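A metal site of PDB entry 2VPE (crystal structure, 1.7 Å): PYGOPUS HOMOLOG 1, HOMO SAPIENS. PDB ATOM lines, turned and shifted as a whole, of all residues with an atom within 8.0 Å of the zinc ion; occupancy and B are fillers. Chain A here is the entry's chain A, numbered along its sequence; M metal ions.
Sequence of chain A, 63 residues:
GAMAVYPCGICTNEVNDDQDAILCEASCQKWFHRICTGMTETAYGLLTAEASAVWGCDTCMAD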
ATOM      1  N   GLY A   9     -24.250  -9.851  32.789  1.00  0.00           N
ATOM      2  CA  GLY A   9     -22.816 -10.152  32.854  1.00  0.00           C
ATOM      3  C   GLY A   9     -22.156  -9.577  34.122  1.00  0.00           C
ATOM      4  O   GLY A   9     -21.119 -10.079  34.566  1.00  0.00           O
ATOM      5  N   LEU A  23     -25.890  -5.911  24.585  1.00  0.00           N
ATOM      6  CA  LEU A  23     -25.241  -7.188  24.338  1.00  0.00           C
ATOM      7  C   LEU A  23     -23.754  -6.951  24.074  1.00  0.00           C
ATOM      8  O   LEU A  23     -23.417  -6.078  23.250  1.00  0.00           O
ATOM      9  CB  LEU A  23     -25.884  -7.843  23.106  1.00  0.00           C
ATOM     10  CG  LEU A  23     -25.276  -9.186  22.712  1.00  0.00           C
ATOM     11  CD1 LEU A  23     -25.411 -10.217  23.817  1.00  0.00           C
ATOM     12  CD2 LEU A  23     -25.977  -9.636  21.416  1.00  0.00           C
ATOM     13  N   CYS A  24     -22.883  -7.695  24.749  1.00  0.00           N
ATOM     14  CA  CYS A  24     -21.456  -7.627  24.485  1.00  0.00           C
ATOM     15  C   CYS A  24     -21.207  -8.360  23.164  1.00  0.00           C
ATOM     16  O   CYS A  24     -20.940  -9.560  23.167  1.00  0.00           O
ATOM     17  CB  CYS A  24     -20.625  -8.256  25.578  1.00  0.00           C
ATOM     18  SG  CYS A  24     -18.847  -8.096  25.275  1.00  0.00           S
ATOM     19  N   GLU A  25     -21.365  -7.645  22.068  1.00  0.00           N
ATOM     20  CA  GLU A  25     -21.139  -8.253  20.733  1.00  0.00           C
ATOM     21  C   GLU A  25     -19.662  -8.344  20.387  1.00  0.00           C
ATOM     22  O   GLU A  25     -19.271  -9.075  19.456  1.00  0.00           O
ATOM     23  CB  GLU A  25     -21.903  -7.480  19.665  1.00  0.00           C
ATOM     24  CG  GLU A  25     -23.393  -7.593  19.772  1.00  0.00           C
ATOM     25  CD  GLU A  25     -24.096  -6.744  18.744  1.00  0.00           C
ATOM     26  OE1 GLU A  25     -24.573  -7.316  17.726  1.00  0.00           O
ATOM     27  OE2 GLU A  25     -24.161  -5.500  18.932  1.00  0.00           O
ATOM     28  N   ALA A  26     -18.838  -7.606  21.121  1.00  0.00           N
ATOM     29  CA  ALA A  26     -17.378  -7.632  20.917  1.00  0.00           C
ATOM     30  C   ALA A  26     -16.800  -9.021  21.167  1.00  0.00           C
ATOM     31  O   ALA A  26     -15.839  -9.427  20.489  1.00  0.00           O
ATOM     32  CB  ALA A  26     -16.683  -6.620  21.791  1.00  0.00           C
ATOM     33  N   SER A  27     -17.376  -9.737  22.130  1.00  0.00           N
ATOM     34  CA  SER A  27     -16.823 -11.018  22.510  1.00  0.00           C
ATOM     35  C   SER A  27     -17.748 -11.977  23.242  1.00  0.00           C
ATOM     36  O   SER A  27     -18.146 -13.009  22.682  1.00  0.00           O
ATOM     37  CB  SER A  27     -15.552 -10.813  23.339  1.00  0.00           C
ATOM     38  OG  SER A  27     -14.803 -12.019  23.382  1.00  0.00           O
ATOM     39  N   CYS A  28     -18.071 -11.674  24.495  1.00  0.00           N
ATOM     40  CA  CYS A  28     -18.612 -12.720  25.377  1.00  0.00           C
ATOM     41  C   CYS A  28     -20.087 -13.021  25.166  1.00  0.00           C
ATOM     42  O   CYS A  28     -20.577 -14.030  25.661  1.00  0.00           O
ATOM     43  CB  CYS A  28     -18.323 -12.402  26.857  1.00  0.00           C
ATOM     44  SG  CYS A  28     -19.316 -11.007  27.554  1.00  0.00           S
ATOM     45  N   GLN A  29     -20.790 -12.157  24.443  1.00  0.00           N
ATOM     46  CA  GLN A  29     -22.222 -12.339  24.131  1.00  0.00           C
ATOM     47  C   GLN A  29     -23.167 -12.448  25.344  1.00  0.00           C
ATOM     48  O   GLN A  29     -24.267 -12.999  25.218  1.00  0.00           O
ATOM     49  CB  GLN A  29     -22.473 -13.519  23.164  1.00  0.00           C
ATOM     50  CG  GLN A  29     -21.524 -13.621  21.993  1.00  0.00           C
ATOM     51  CD  GLN A  29     -21.557 -12.408  21.108  1.00  0.00           C
ATOM     52  OE1 GLN A  29     -22.629 -11.851  20.834  1.00  0.00           O
ATOM     53  NE2 GLN A  29     -20.382 -11.974  20.655  1.00  0.00           N
ATOM     54  N   LYS A  30     -22.750 -11.943  26.492  1.00  0.00           N
ATOM     55  CA  LYS A  30     -23.679 -11.761  27.611  1.00  0.00           C
ATOM     56  C   LYS A  30     -24.410 -10.433  27.435  1.00  0.00           C
ATOM     57  O   LYS A  30     -23.851  -9.490  26.841  1.00  0.00           O
ATOM     58  CB  LYS A  30     -22.918 -11.734  28.921  1.00  0.00           C
ATOM     59  CG  LYS A  30     -22.097 -13.002  29.222  1.00  0.00           C
ATOM     60  CD  LYS A  30     -21.348 -12.838  30.526  1.00  0.00           C
ATOM     61  CE  LYS A  30     -20.288 -13.946  30.761  1.00  0.00           C
ATOM     62  NZ  LYS A  30     -19.379 -13.721  31.955  1.00  0.00           N
ATOM     63  N   TRP A  31     -25.632 -10.378  27.956  1.00  0.00           N
ATOM     64  CA  TRP A  31     -26.362  -9.123  28.103  1.00  0.00           C
ATOM     65  C   TRP A  31     -25.941  -8.425  29.403  1.00  0.00           C
ATOM     66  O   TRP A  31     -25.620  -9.104  30.405  1.00  0.00           O
ATOM     67  CB  TRP A  31     -27.849  -9.387  28.106  1.00  0.00           C
ATOM     68  CG  TRP A  31     -28.393  -9.575  26.734  1.00  0.00           C
ATOM     69  CD1 TRP A  31     -28.505 -10.748  26.049  1.00  0.00           C
ATOM     70  CD2 TRP A  31     -28.857  -8.550  25.867  1.00  0.00           C
ATOM     71  NE1 TRP A  31     -29.046 -10.516  24.810  1.00  0.00           N
ATOM     72  CE2 TRP A  31     -29.262  -9.174  24.660  1.00  0.00           C
ATOM     73  CE3 TRP A  31     -28.987  -7.154  25.987  1.00  0.00           C
ATOM     74  CZ2 TRP A  31     -29.782  -8.450  23.570  1.00  0.00           C
ATOM     75  CZ3 TRP A  31     -29.523  -6.428  24.915  1.00  0.00           C
ATOM     76  CH2 TRP A  31     -29.895  -7.077  23.712  1.00  0.00           C
ATOM     77  N   PHE A  32     -25.936  -7.089  29.371  1.00  0.00           N
ATOM     78  CA  PHE A  32     -25.548  -6.312  30.543  1.00  0.00           C
ATOM     79  C   PHE A  32     -26.564  -5.196  30.714  1.00  0.00           C
ATOM     80  O   PHE A  32     -26.834  -4.468  29.763  1.00  0.00           O
ATOM     81  CB  PHE A  32     -24.188  -5.658  30.317  1.00  0.00           C
ATOM     82  CG  PHE A  32     -23.026  -6.631  30.280  1.00  0.00           C
ATOM     83  CD1 PHE A  32     -22.150  -6.700  31.363  1.00  0.00           C
ATOM     84  CD2 PHE A  32     -22.803  -7.425  29.173  1.00  0.00           C
ATOM     85  CE1 PHE A  32     -21.059  -7.599  31.349  1.00  0.00           C
ATOM     86  CE2 PHE A  32     -21.700  -8.307  29.144  1.00  0.00           C
ATOM     87  CZ  PHE A  32     -20.839  -8.386  30.211  1.00  0.00           C
ATOM     88  N   TRP A  55     -20.699  -2.956  21.046  1.00  0.00           N
ATOM     89  CA  TRP A  55     -20.125  -2.655  22.332  1.00  0.00           C
ATOM     90  C   TRP A  55     -19.457  -3.907  22.898  1.00  0.00           C
ATOM     91  O   TRP A  55     -19.908  -5.049  22.636  1.00  0.00           O
ATOM     92  CB  TRP A  55     -21.241  -2.151  23.279  1.00  0.00           C
ATOM     93  CG  TRP A  55     -20.860  -2.006  24.688  1.00  0.00           C
ATOM     94  CD1 TRP A  55     -20.198  -0.957  25.270  1.00  0.00           C
ATOM     95  CD2 TRP A  55     -21.122  -2.945  25.745  1.00  0.00           C
ATOM     96  NE1 TRP A  55     -20.025  -1.183  26.606  1.00  0.00           N
ATOM     97  CE2 TRP A  55     -20.567  -2.392  26.936  1.00  0.00           C
ATOM     98  CE3 TRP A  55     -21.718  -4.209  25.800  1.00  0.00           C
ATOM     99  CZ2 TRP A  55     -20.631  -3.059  28.156  1.00  0.00           C
ATOM    100  CZ3 TRP A  55     -21.804  -4.863  27.033  1.00  0.00           C
ATOM    101  CH2 TRP A  55     -21.239  -4.295  28.177  1.00  0.00           C
ATOM    102  N   GLY A  56     -18.367  -3.685  23.636  1.00  0.00           N
ATOM    103  CA  GLY A  56     -17.696  -4.711  24.427  1.00  0.00           C
ATOM    104  C   GLY A  56     -17.631  -4.359  25.885  1.00  0.00           C
ATOM    105  O   GLY A  56     -17.362  -3.204  26.235  1.00  0.00           O
ATOM    106  N   CYS A  57     -17.841  -5.347  26.764  1.00  0.00           N
ATOM    107  CA  CYS A  57     -17.779  -5.118  28.203  1.00  0.00           C
ATOM    108  C   CYS A  57     -16.322  -4.859  28.606  1.00  0.00           C
ATOM    109  O   CYS A  57     -15.394  -5.151  27.827  1.00  0.00           O
ATOM    110  CB  CYS A  57     -18.368  -6.268  29.001  1.00  0.00           C
ATOM    111  SG  CYS A  57     -17.323  -7.740  28.927  1.00  0.00           S
ATOM    112  N   ASP A  58     -16.134  -4.319  29.800  1.00  0.00           N
ATOM    113  CA  ASP A  58     -14.799  -3.968  30.276  1.00  0.00           C
ATOM    114  C   ASP A  58     -13.826  -5.151  30.249  1.00  0.00           C
ATOM    115  O   ASP A  58     -12.664  -4.978  29.893  1.00  0.00           O
ATOM    116  CB  ASP A  58     -14.864  -3.363  31.669  1.00  0.00           C
ATOM    117  CG  ASP A  58     -15.529  -1.996  31.679  1.00  0.00           C
ATOM    118  OD1 ASP A  58     -15.782  -1.406  30.586  1.00  0.00           O
ATOM    119  OD2 ASP A  58     -15.799  -1.491  32.807  1.00  0.00           O
ATOM    120  N   THR A  59     -14.318  -6.333  30.638  1.00  0.00           N
ATOM    121  CA  THR A  59     -13.495  -7.558  30.653  1.00  0.00           C
ATOM    122  C   THR A  59     -13.024  -7.920  29.253  1.00  0.00           C
ATOM    123  O   THR A  59     -11.834  -8.154  29.031  1.00  0.00           O
ATOM    124  CB  THR A  59     -14.259  -8.715  31.298  1.00  0.00           C
ATOM    125  OG1 THR A  59     -14.493  -8.392  32.670  1.00  0.00           O
ATOM    126  CG2 THR A  59     -13.471 -10.037  31.214  1.00  0.00           C
ATOM    127  N   CYS A  60     -13.959  -7.950  28.304  1.00  0.00           N
ATOM    128  CA  CYS A  60     -13.659  -8.278  26.923  1.00  0.00           C
ATOM    129  C   CYS A  60     -12.756  -7.243  26.249  1.00  0.00           C
ATOM    130  O   CYS A  60     -11.883  -7.622  25.438  1.00  0.00           O
ATOM    131  CB  CYS A  60     -14.949  -8.443  26.132  1.00  0.00           C
ATOM    132  SG  CYS A  60     -15.791 -10.014  26.524  1.00  0.00           S
ATOM    133  N   MET A  61     -12.954  -5.961  26.550  1.00  0.00           N
ATOM    134  CA  MET A  61     -12.151  -4.897  25.928  1.00  0.00           C
ATOM    135  C   MET A  61     -10.716  -4.924  26.439  1.00  0.00           C
ATOM    136  O   MET A  61      -9.776  -4.642  25.692  1.00  0.00           O
ATOM    137  CB  MET A  61     -12.785  -3.520  26.126  1.00  0.00           C
ATOM    138  CG  MET A  61     -14.107  -3.342  25.407  1.00  0.00           C
ATOM    139  SD  MET A  61     -14.078  -3.665  23.629  1.00  0.00           S
ATOM    140  CE  MET A  61     -13.105  -2.260  23.048  1.00  0.00           C
ATOM    141  N   ASP A  63      -9.103  -7.619  27.307  1.00  0.00           N
ATOM    142  CA  ASP A  63      -8.437  -8.768  26.660  1.00  0.00           C
ATOM    143  C   ASP A  63      -7.789  -8.357  25.345  1.00  0.00           C
ATOM    144  O   ASP A  63      -8.435  -7.750  24.486  1.00  0.00           O
ATOM    145  CB  ASP A  63      -9.432  -9.906  26.400  1.00  0.00           C
ATOM    146  CG  ASP A  63     -10.013 -10.496  27.687  1.00  0.00           C
ATOM    147  OD1 ASP A  63      -9.310 -10.546  28.721  1.00  0.00           O
ATOM    148  OD2 ASP A  63     -11.183 -10.927  27.647  1.00  0.00           O
HETATM  149 ZN    ZN M   1     -17.911  -9.150  27.076  1.00  0.00          ZN
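The backbone carbonyl oxygen of Cys 24 lies within hydrogen-bond range of the backbone NH of Gln 29, at 2.9 Å.
N of Cys 24 is in hydrogen-bond range of O of Lys 30 (2.9 Å).
N of Lys 30 sits close to SG of Cys 28, 3.7 Å away.
The side-chain sulfur (SG) of Cys 57 sits close to the backbone NH (N) of Thr 59, 3.7 Å away.
Of the 19 residues printed, 4 come within 4 Å of the zinc ion.
Along chain A the residues within 4 Å of the zinc ion span positions 24 to 60.
The nearest printed residue that does not touch the zinc ion is Phe 32 (4.4 Å).
The zinc ion is bound by SG of Cys 24.
The side-chain sulfur (SG) of Cys 60 binds the zinc ion, 2.4 Å away.
The side-chain sulfur (SG) of Cys 28 binds the zinc ion (2.4 Å).
The zinc ion is bound by SG of Cys 57 (2.4 Å).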
